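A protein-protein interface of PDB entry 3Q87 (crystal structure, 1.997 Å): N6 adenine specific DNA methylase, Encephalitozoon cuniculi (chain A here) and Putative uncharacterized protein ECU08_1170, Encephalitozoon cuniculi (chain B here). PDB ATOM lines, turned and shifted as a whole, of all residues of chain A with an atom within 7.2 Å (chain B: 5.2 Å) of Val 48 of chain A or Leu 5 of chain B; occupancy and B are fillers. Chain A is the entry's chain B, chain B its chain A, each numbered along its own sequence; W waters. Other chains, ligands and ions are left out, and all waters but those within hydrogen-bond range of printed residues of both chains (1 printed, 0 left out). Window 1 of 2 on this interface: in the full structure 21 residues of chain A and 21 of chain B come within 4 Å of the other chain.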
ATOM      1  N   ILE A  26     -13.887  -1.710   6.387  1.00  0.00           N
ATOM      2  CA  ILE A  26     -13.178  -2.929   6.025  1.00  0.00           C
ATOM      3  C   ILE A  26     -13.349  -3.075   4.518  1.00  0.00           C
ATOM      4  O   ILE A  26     -14.458  -3.196   4.030  1.00  0.00           O
ATOM      5  CB  ILE A  26     -13.716  -4.180   6.758  1.00  0.00           C
ATOM      6  CG1 ILE A  26     -13.494  -4.056   8.267  1.00  0.00           C
ATOM      7  CG2 ILE A  26     -13.005  -5.444   6.258  1.00  0.00           C
ATOM      8  CD1 ILE A  26     -14.114  -5.234   9.062  1.00  0.00           C
ATOM      9  N   VAL A  27     -12.245  -3.007   3.781  1.00  0.00           N
ATOM     10  CA  VAL A  27     -12.314  -2.928   2.326  1.00  0.00           C
ATOM     11  C   VAL A  27     -11.625  -4.123   1.710  1.00  0.00           C
ATOM     12  O   VAL A  27     -10.522  -4.513   2.116  1.00  0.00           O
ATOM     13  CB  VAL A  27     -11.620  -1.657   1.778  1.00  0.00           C
ATOM     14  CG1 VAL A  27     -11.733  -1.586   0.246  1.00  0.00           C
ATOM     15  CG2 VAL A  27     -12.208  -0.419   2.417  1.00  0.00           C
ATOM     16  N   LEU A  28     -12.289  -4.716   0.734  1.00  0.00           N
ATOM     17  CA  LEU A  28     -11.698  -5.816  -0.001  1.00  0.00           C
ATOM     18  C   LEU A  28     -11.157  -5.258  -1.304  1.00  0.00           C
ATOM     19  O   LEU A  28     -11.937  -4.777  -2.131  1.00  0.00           O
ATOM     20  CB  LEU A  28     -12.753  -6.880  -0.297  1.00  0.00           C
ATOM     21  CG  LEU A  28     -12.235  -8.165  -0.953  1.00  0.00           C
ATOM     22  CD1 LEU A  28     -11.510  -9.046   0.061  1.00  0.00           C
ATOM     23  CD2 LEU A  28     -13.384  -8.940  -1.594  1.00  0.00           C
ATOM     24  N   ASP A  29      -9.834  -5.292  -1.464  1.00  0.00           N
ATOM     25  CA  ASP A  29      -9.195  -4.926  -2.732  1.00  0.00           C
ATOM     26  C   ASP A  29      -9.113  -6.201  -3.568  1.00  0.00           C
ATOM     27  O   ASP A  29      -8.192  -7.003  -3.420  1.00  0.00           O
ATOM     28  CB  ASP A  29      -7.788  -4.359  -2.490  1.00  0.00           C
ATOM     29  CG  ASP A  29      -7.030  -4.057  -3.789  1.00  0.00           C
ATOM     30  OD1 ASP A  29      -7.652  -4.070  -4.884  1.00  0.00           O
ATOM     31  OD2 ASP A  29      -5.801  -3.800  -3.714  1.00  0.00           O
ATOM     32  N   LEU A  30     -10.104  -6.394  -4.426  1.00  0.00           N
ATOM     33  CA  LEU A  30     -10.229  -7.606  -5.219  1.00  0.00           C
ATOM     34  C   LEU A  30      -9.390  -7.479  -6.491  1.00  0.00           C
ATOM     35  O   LEU A  30      -9.495  -6.478  -7.188  1.00  0.00           O
ATOM     36  CB  LEU A  30     -11.706  -7.786  -5.577  1.00  0.00           C
ATOM     37  CG  LEU A  30     -12.174  -9.050  -6.286  1.00  0.00           C
ATOM     38  CD1 LEU A  30     -11.860 -10.257  -5.448  1.00  0.00           C
ATOM     39  CD2 LEU A  30     -13.681  -8.968  -6.549  1.00  0.00           C
ATOM     40  N   THR A  32      -5.975  -7.509  -6.411  1.00  0.00           N
ATOM     41  CA  THR A  32      -5.048  -6.534  -5.878  1.00  0.00           C
ATOM     42  C   THR A  32      -3.778  -6.460  -6.694  1.00  0.00           C
ATOM     43  O   THR A  32      -3.096  -5.440  -6.676  1.00  0.00           O
ATOM     44  CB  THR A  32      -4.665  -6.862  -4.411  1.00  0.00           C
ATOM     45  OG1 THR A  32      -3.763  -5.874  -3.918  1.00  0.00           O
ATOM     46  CG2 THR A  32      -4.018  -8.227  -4.315  1.00  0.00           C
ATOM     47  N   THR A  38      -4.233  -1.132  -2.673  1.00  0.00           N
ATOM     48  CA  THR A  38      -4.138  -1.477  -1.255  1.00  0.00           C
ATOM     49  C   THR A  38      -3.286  -0.458  -0.490  1.00  0.00           C
ATOM     50  O   THR A  38      -3.647  -0.014   0.600  1.00  0.00           O
ATOM     51  CB  THR A  38      -3.538  -2.900  -1.042  1.00  0.00           C
ATOM     52  OG1 THR A  38      -4.495  -3.890  -1.429  1.00  0.00           O
ATOM     53  CG2 THR A  38      -3.157  -3.123   0.438  1.00  0.00           C
ATOM     54  N   LEU A  41      -5.417   2.571   0.059  1.00  0.00           N
ATOM     55  CA  LEU A  41      -6.551   2.221   0.915  1.00  0.00           C
ATOM     56  C   LEU A  41      -6.182   1.985   2.376  1.00  0.00           C
ATOM     57  O   LEU A  41      -6.957   2.289   3.270  1.00  0.00           O
ATOM     58  CB  LEU A  41      -7.239   0.959   0.388  1.00  0.00           C
ATOM     59  CG  LEU A  41      -8.022   1.113  -0.912  1.00  0.00           C
ATOM     60  CD1 LEU A  41      -8.555  -0.220  -1.383  1.00  0.00           C
ATOM     61  CD2 LEU A  41      -9.151   2.098  -0.713  1.00  0.00           C
ATOM     62  N   THR A  46      -9.040  -0.736   6.984  1.00  0.00           N
ATOM     63  CA  THR A  46      -8.478  -2.074   7.083  1.00  0.00           C
ATOM     64  C   THR A  46      -8.766  -2.830   5.793  1.00  0.00           C
ATOM     65  O   THR A  46      -9.916  -2.950   5.374  1.00  0.00           O
ATOM     66  CB  THR A  46      -9.014  -2.849   8.280  1.00  0.00           C
ATOM     67  OG1 THR A  46      -8.719  -2.118   9.478  1.00  0.00           O
ATOM     68  CG2 THR A  46      -8.333  -4.227   8.346  1.00  0.00           C
ATOM     69  N   VAL A  47      -7.708  -3.318   5.158  1.00  0.00           N
ATOM     70  CA  VAL A  47      -7.828  -3.874   3.815  1.00  0.00           C
ATOM     71  C   VAL A  47      -7.471  -5.351   3.780  1.00  0.00           C
ATOM     72  O   VAL A  47      -6.455  -5.761   4.322  1.00  0.00           O
ATOM     73  CB  VAL A  47      -6.896  -3.139   2.823  1.00  0.00           C
ATOM     74  CG1 VAL A  47      -7.089  -3.681   1.397  1.00  0.00           C
ATOM     75  CG2 VAL A  47      -7.121  -1.612   2.880  1.00  0.00           C
ATOM     76  N   VAL A  48      -8.325  -6.143   3.143  1.00  0.00           N
ATOM     77  CA  VAL A  48      -7.980  -7.493   2.757  1.00  0.00           C
ATOM     78  C   VAL A  48      -7.731  -7.472   1.257  1.00  0.00           C
ATOM     79  O   VAL A  48      -8.534  -6.952   0.514  1.00  0.00           O
ATOM     80  CB  VAL A  48      -9.106  -8.487   3.096  1.00  0.00           C
ATOM     81  CG1 VAL A  48      -8.698  -9.916   2.686  1.00  0.00           C
ATOM     82  CG2 VAL A  48      -9.391  -8.421   4.587  1.00  0.00           C
ATOM     83  N   SER A  49      -6.601  -8.013   0.818  1.00  0.00           N
ATOM     84  CA  SER A  49      -6.254  -7.958  -0.596  1.00  0.00           C
ATOM     85  C   SER A  49      -6.168  -9.353  -1.200  1.00  0.00           C
ATOM     86  O   SER A  49      -5.478 -10.228  -0.662  1.00  0.00           O
ATOM     87  CB  SER A  49      -4.936  -7.208  -0.763  1.00  0.00           C
ATOM     88  OG  SER A  49      -4.978  -6.006  -0.017  1.00  0.00           O
ATOM     89  N   THR A  50      -6.885  -9.566  -2.304  1.00  0.00           N
ATOM     90  CA  THR A  50      -6.977 -10.899  -2.899  1.00  0.00           C
ATOM     91  C   THR A  50      -6.652 -10.885  -4.379  1.00  0.00           C
ATOM     92  O   THR A  50      -6.857  -9.882  -5.049  1.00  0.00           O
ATOM     93  CB  THR A  50      -8.386 -11.533  -2.731  1.00  0.00           C
ATOM     94  OG1 THR A  50      -9.290 -10.937  -3.666  1.00  0.00           O
ATOM     95  CG2 THR A  50      -8.916 -11.344  -1.308  1.00  0.00           C
ATOM     96  N   GLY A  63       0.419  -6.412   2.670  1.00  0.00           N
ATOM     97  CA  GLY A  63      -0.947  -6.313   3.128  1.00  0.00           C
ATOM     98  C   GLY A  63      -1.434  -7.629   3.675  1.00  0.00           C
ATOM     99  O   GLY A  63      -0.641  -8.484   4.060  1.00  0.00           O
ATOM    100  N   ASN A  64      -2.746  -7.792   3.707  1.00  0.00           N
ATOM    101  CA  ASN A  64      -3.338  -9.028   4.197  1.00  0.00           C
ATOM    102  C   ASN A  64      -3.789  -9.835   2.991  1.00  0.00           C
ATOM    103  O   ASN A  64      -4.818  -9.552   2.389  1.00  0.00           O
ATOM    104  CB  ASN A  64      -4.476  -8.681   5.140  1.00  0.00           C
ATOM    105  CG  ASN A  64      -4.012  -7.753   6.259  1.00  0.00           C
ATOM    106  OD1 ASN A  64      -3.184  -8.135   7.083  1.00  0.00           O
ATOM    107  ND2 ASN A  64      -4.510  -6.530   6.266  1.00  0.00           N
ATOM    108  N   LEU A  65      -2.973 -10.816   2.626  1.00  0.00           N
ATOM    109  CA  LEU A  65      -3.048 -11.430   1.315  1.00  0.00           C
ATOM    110  C   LEU A  65      -3.809 -12.750   1.313  1.00  0.00           C
ATOM    111  O   LEU A  65      -3.547 -13.638   2.135  1.00  0.00           O
ATOM    112  CB  LEU A  65      -1.636 -11.626   0.760  1.00  0.00           C
ATOM    113  CG  LEU A  65      -0.776 -10.351   0.761  1.00  0.00           C
ATOM    114  CD1 LEU A  65       0.535 -10.605   0.045  1.00  0.00           C
ATOM    115  CD2 LEU A  65      -1.505  -9.171   0.116  1.00  0.00           C
ATOM    116  N   VAL A  66      -4.754 -12.856   0.383  1.00  0.00           N
ATOM    117  CA  VAL A  66      -5.501 -14.081   0.156  1.00  0.00           C
ATOM    118  C   VAL A  66      -5.460 -14.420  -1.321  1.00  0.00           C
ATOM    119  O   VAL A  66      -5.782 -13.577  -2.160  1.00  0.00           O
ATOM    120  CB  VAL A  66      -6.975 -13.921   0.590  1.00  0.00           C
ATOM    121  CG1 VAL A  66      -7.714 -15.272   0.502  1.00  0.00           C
ATOM    122  CG2 VAL A  66      -7.044 -13.349   2.011  1.00  0.00           C
ATOM    123  N   ILE A  74     -14.638 -15.583   0.702  1.00  0.00           N
ATOM    124  CA  ILE A  74     -14.795 -14.380   1.501  1.00  0.00           C
ATOM    125  C   ILE A  74     -16.181 -14.318   2.121  1.00  0.00           C
ATOM    126  O   ILE A  74     -17.191 -14.487   1.439  1.00  0.00           O
ATOM    127  CB  ILE A  74     -14.568 -13.083   0.648  1.00  0.00           C
ATOM    128  CG1 ILE A  74     -13.193 -13.108  -0.022  1.00  0.00           C
ATOM    129  CG2 ILE A  74     -14.718 -11.830   1.518  1.00  0.00           C
ATOM    130  CD1 ILE A  74     -12.018 -13.340   0.966  1.00  0.00           C
ATOM    131  N   VAL A  79     -17.461  -7.552   5.211  1.00  0.00           N
ATOM    132  CA  VAL A  79     -16.811  -6.524   4.397  1.00  0.00           C
ATOM    133  C   VAL A  79     -17.744  -5.355   4.129  1.00  0.00           C
ATOM    134  O   VAL A  79     -18.906  -5.553   3.752  1.00  0.00           O
ATOM    135  CB  VAL A  79     -16.326  -7.118   3.056  1.00  0.00           C
ATOM    136  CG1 VAL A  79     -15.755  -6.020   2.124  1.00  0.00           C
ATOM    137  CG2 VAL A  79     -15.312  -8.217   3.321  1.00  0.00           C
ATOM    138  N   VAL A  81     -16.811  -2.592   1.899  1.00  0.00           N
ATOM    139  CA  VAL A  81     -16.629  -2.139   0.524  1.00  0.00           C
ATOM    140  C   VAL A  81     -15.748  -3.104  -0.258  1.00  0.00           C
ATOM    141  O   VAL A  81     -14.759  -3.641   0.272  1.00  0.00           O
ATOM    142  CB  VAL A  81     -15.917  -0.756   0.490  1.00  0.00           C
ATOM    143  CG1 VAL A  81     -15.591  -0.314  -0.948  1.00  0.00           C
ATOM    144  CG2 VAL A  81     -16.740   0.287   1.219  1.00  0.00           C
ATOM    145  N   MET B   1      -0.751 -14.487   7.469  1.00  0.00           N
ATOM    146  CA  MET B   1      -2.081 -13.986   7.797  1.00  0.00           C
ATOM    147  C   MET B   1      -2.252 -13.653   9.275  1.00  0.00           C
ATOM    148  O   MET B   1      -1.914 -14.440  10.160  1.00  0.00           O
ATOM    149  CB  MET B   1      -3.181 -14.958   7.348  1.00  0.00           C
ATOM    150  CG  MET B   1      -3.452 -16.087   8.299  1.00  0.00           C
ATOM    151  SD  MET B   1      -5.199 -16.606   8.320  1.00  0.00           S
ATOM    152  CE  MET B   1      -5.920 -15.401   9.427  1.00  0.00           C
ATOM    153  N   LYS B   2      -2.796 -12.473   9.520  1.00  0.00           N
ATOM    154  CA  LYS B   2      -3.127 -12.040  10.861  1.00  0.00           C
ATOM    155  C   LYS B   2      -4.476 -12.632  11.273  1.00  0.00           C
ATOM    156  O   LYS B   2      -5.374 -12.776  10.455  1.00  0.00           O
ATOM    157  CB  LYS B   2      -3.166 -10.518  10.917  1.00  0.00           C
ATOM    158  CG  LYS B   2      -1.883  -9.865  10.417  1.00  0.00           C
ATOM    159  CD  LYS B   2      -2.047  -8.363  10.352  1.00  0.00           C
ATOM    160  CE  LYS B   2      -0.734  -7.676  10.005  1.00  0.00           C
ATOM    161  NZ  LYS B   2      -0.904  -6.194   9.999  1.00  0.00           N
ATOM    162  N   PRO B   3      -4.606 -13.012  12.547  1.00  0.00           N
ATOM    163  CA  PRO B   3      -5.815 -13.716  12.990  1.00  0.00           C
ATOM    164  C   PRO B   3      -7.133 -12.950  12.803  1.00  0.00           C
ATOM    165  O   PRO B   3      -8.186 -13.588  12.792  1.00  0.00           O
ATOM    166  CB  PRO B   3      -5.524 -13.992  14.471  1.00  0.00           C
ATOM    167  CG  PRO B   3      -4.011 -14.155  14.498  1.00  0.00           C
ATOM    168  CD  PRO B   3      -3.499 -13.139  13.513  1.00  0.00           C
ATOM    169  N   PHE B   4      -7.107 -11.630  12.637  1.00  0.00           N
ATOM    170  CA  PHE B   4      -8.372 -10.919  12.413  1.00  0.00           C
ATOM    171  C   PHE B   4      -9.043 -11.390  11.131  1.00  0.00           C
ATOM    172  O   PHE B   4     -10.260 -11.239  10.973  1.00  0.00           O
ATOM    173  CB  PHE B   4      -8.192  -9.396  12.408  1.00  0.00           C
ATOM    174  CG  PHE B   4      -7.826  -8.825  11.065  1.00  0.00           C
ATOM    175  CD1 PHE B   4      -8.809  -8.354  10.209  1.00  0.00           C
ATOM    176  CD2 PHE B   4      -6.508  -8.760  10.665  1.00  0.00           C
ATOM    177  CE1 PHE B   4      -8.479  -7.825   8.973  1.00  0.00           C
ATOM    178  CE2 PHE B   4      -6.165  -8.225   9.433  1.00  0.00           C
ATOM    179  CZ  PHE B   4      -7.157  -7.762   8.584  1.00  0.00           C
ATOM    180  N   LEU B   5      -8.258 -11.978  10.227  1.00  0.00           N
ATOM    181  CA  LEU B   5      -8.812 -12.495   8.965  1.00  0.00           C
ATOM    182  C   LEU B   5      -9.835 -13.605   9.209  1.00  0.00           C
ATOM    183  O   LEU B   5     -10.677 -13.879   8.358  1.00  0.00           O
ATOM    184  CB  LEU B   5      -7.712 -12.991   8.025  1.00  0.00           C
ATOM    185  CG  LEU B   5      -7.012 -11.898   7.208  1.00  0.00           C
ATOM    186  CD1 LEU B   5      -6.235 -12.505   6.053  1.00  0.00           C
ATOM    187  CD2 LEU B   5      -8.037 -10.918   6.683  1.00  0.00           C
ATOM    188  N   LEU B   6      -9.767 -14.238  10.380  1.00  0.00           N
ATOM    189  CA  LEU B   6     -10.743 -15.267  10.725  1.00  0.00           C
ATOM    190  C   LEU B   6     -12.168 -14.720  10.816  1.00  0.00           C
ATOM    191  O   LEU B   6     -13.123 -15.496  10.835  1.00  0.00           O
ATOM    192  CB  LEU B   6     -10.373 -15.975  12.026  1.00  0.00           C
ATOM    193  CG  LEU B   6      -9.469 -17.193  11.857  1.00  0.00           C
ATOM    194  CD1 LEU B   6      -9.144 -17.730  13.216  1.00  0.00           C
ATOM    195  CD2 LEU B   6     -10.167 -18.254  11.026  1.00  0.00           C
ATOM    196  N   GLY B   7     -12.320 -13.399  10.889  1.00  0.00           N
ATOM    197  CA  GLY B   7     -13.647 -12.812  10.804  1.00  0.00           C
ATOM    198  C   GLY B   7     -14.145 -12.625   9.373  1.00  0.00           C
ATOM    199  O   GLY B   7     -15.320 -12.337   9.146  1.00  0.00           O
ATOM    200  N   LEU B   8     -13.254 -12.793   8.404  1.00  0.00           N
ATOM    201  CA  LEU B   8     -13.537 -12.402   7.021  1.00  0.00           C
ATOM    202  C   LEU B   8     -13.541 -13.574   6.046  1.00  0.00           C
ATOM    203  O   LEU B   8     -14.078 -13.480   4.939  1.00  0.00           O
ATOM    204  CB  LEU B   8     -12.497 -11.374   6.557  1.00  0.00           C
ATOM    205  CG  LEU B   8     -12.763  -9.953   7.057  1.00  0.00           C
ATOM    206  CD1 LEU B   8     -11.488  -9.215   7.374  1.00  0.00           C
ATOM    207  CD2 LEU B   8     -13.586  -9.192   6.031  1.00  0.00           C
ATOM    208  N   LEU B   9     -12.921 -14.675   6.438  1.00  0.00           N
ATOM    209  CA  LEU B   9     -12.791 -15.804   5.531  1.00  0.00           C
ATOM    210  C   LEU B   9     -13.898 -16.807   5.795  1.00  0.00           C
ATOM    211  O   LEU B   9     -14.400 -16.888   6.899  1.00  0.00           O
ATOM    212  CB  LEU B   9     -11.429 -16.469   5.695  1.00  0.00           C
ATOM    213  CG  LEU B   9     -10.182 -15.790   5.114  1.00  0.00           C
ATOM    214  CD1 LEU B   9      -8.927 -16.350   5.747  1.00  0.00           C
ATOM    215  CD2 LEU B   9     -10.132 -15.970   3.610  1.00  0.00           C
ATOM    216  N   VAL B 116      -2.905 -16.652   2.400  1.00  0.00           N
ATOM    217  CA  VAL B 116      -3.936 -17.685   2.523  1.00  0.00           C
ATOM    218  C   VAL B 116      -4.346 -18.196   1.142  1.00  0.00           C
ATOM    219  O   VAL B 116      -4.771 -17.443   0.268  1.00  0.00           O
ATOM    220  CB  VAL B 116      -5.184 -17.195   3.258  1.00  0.00           C
ATOM    221  CG1 VAL B 116      -6.216 -18.344   3.394  1.00  0.00           C
ATOM    222  CG2 VAL B 116      -4.810 -16.619   4.635  1.00  0.00           C
HETATM  223  O   HOH W   1      -2.935 -10.967   7.126  1.00  0.00           O
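The backbone NH (N) of Val 116 of chain B is in hydrogen-bond range of the backbone carbonyl oxygen (O) of Leu 65 of chain A (3.1 Å).
The backbone carbonyl oxygen of Ile 26 of chain A sits at hydrogen-bond distance from the backbone NH of Val 81 of chain A (3.2 Å). The backbone carbonyl oxygen (O) of Thr 46 of chain A is in hydrogen-bond range of the backbone NH (N) of Val 27 of chain A (2.8 Å). N of Val 48 of chain A lies within hydrogen-bond range of O of Val 27 of chain A (2.9 Å). The side-chain amide nitrogen of Asn 64 of chain A sits at hydrogen-bond distance from the backbone carbonyl oxygen of Val 47 of chain A, at 2.9 Å. The backbone NH of Ser 49 of chain A is in hydrogen-bond range of the backbone carbonyl oxygen of Asn 64 of chain A (2.8 Å). The backbone NH (N) of Val 66 of chain A is in hydrogen-bond range of the backbone carbonyl oxygen (O) of Ser 49 of chain A, 2.9 Å away.
Among the printed residues, merely in contact across the chains: Val 79 of chain A with Leu 8 of chain B (3.4 Å), Val 66 of chain A with Val 116 of chain B (3.4 Å), Asn 64 of chain A with Lys 2 of chain B (3.5 Å), Val 48 of chain A with Leu 5 of chain B (3.5 Å), Val 48 of chain A with Leu 8 of chain B (3.6 Å), Ile 74 of chain A with Leu 8 of chain B (3.6 Å), Thr 46 of chain A with Phe 4 of chain B (3.7 Å), Asn 64 of chain A with Phe 4 of chain B (3.7 Å), Ile 26 of chain A with Leu 8 of chain B (3.8 Å) and Val 66 of chain A with Leu 9 of chain B (3.999 Å).
Val 48 of chain A touches just these residues of chain B: Leu 5 and Leu 8. Leu 5 of chain B touches one residue of chain A. Printed residues of chain A within 4 Å of Val 116 of chain B: Leu 65 (3.1 Å) and Val 66 (3.4 Å). Of the printed residues of chain A, Leu 8 of chain B touches Ile 26, Val 48, Ile 74 and Val 79. Of the printed residues of chain B, Leu 65 of chain A touches Val 116 (3.1 Å). Met 1 of chain B touches none of the printed residues of chain A. Pro 3 of chain B touches none of the printed residues of chain A. The nearest residue of chain B that does not touch Val 48 of chain A is Phe 4 of chain B (4.5 Å). The nearest printed residue of chain B that does not touch Asn 64 of chain A is Leu 5 of chain B (4.3 Å).
Of the 10 printed residues of chain B, 6 touch a printed residue of chain A. Hydrophobic or aromatic side chains of chain B that line the printed part of chain A: Phe 4, Leu 5, Leu 8 and Leu 9. Hydrophobic or aromatic side chains of chain A within 4 Å of the printed part of chain B: Ile 26, Val 48, Val 66, Ile 74 and Val 79. Among the printed residues, 11 pairs touch across the chains. Among the printed residues, no Asp or Glu carboxylate lies within 4 Å of a Lys or Arg side-chain nitrogen of the other chain.
Water W1 lies within hydrogen-bond range of the backbone NH of Lys 2 of chain B and the side-chain amide oxygen of Asn 64 of chain A.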
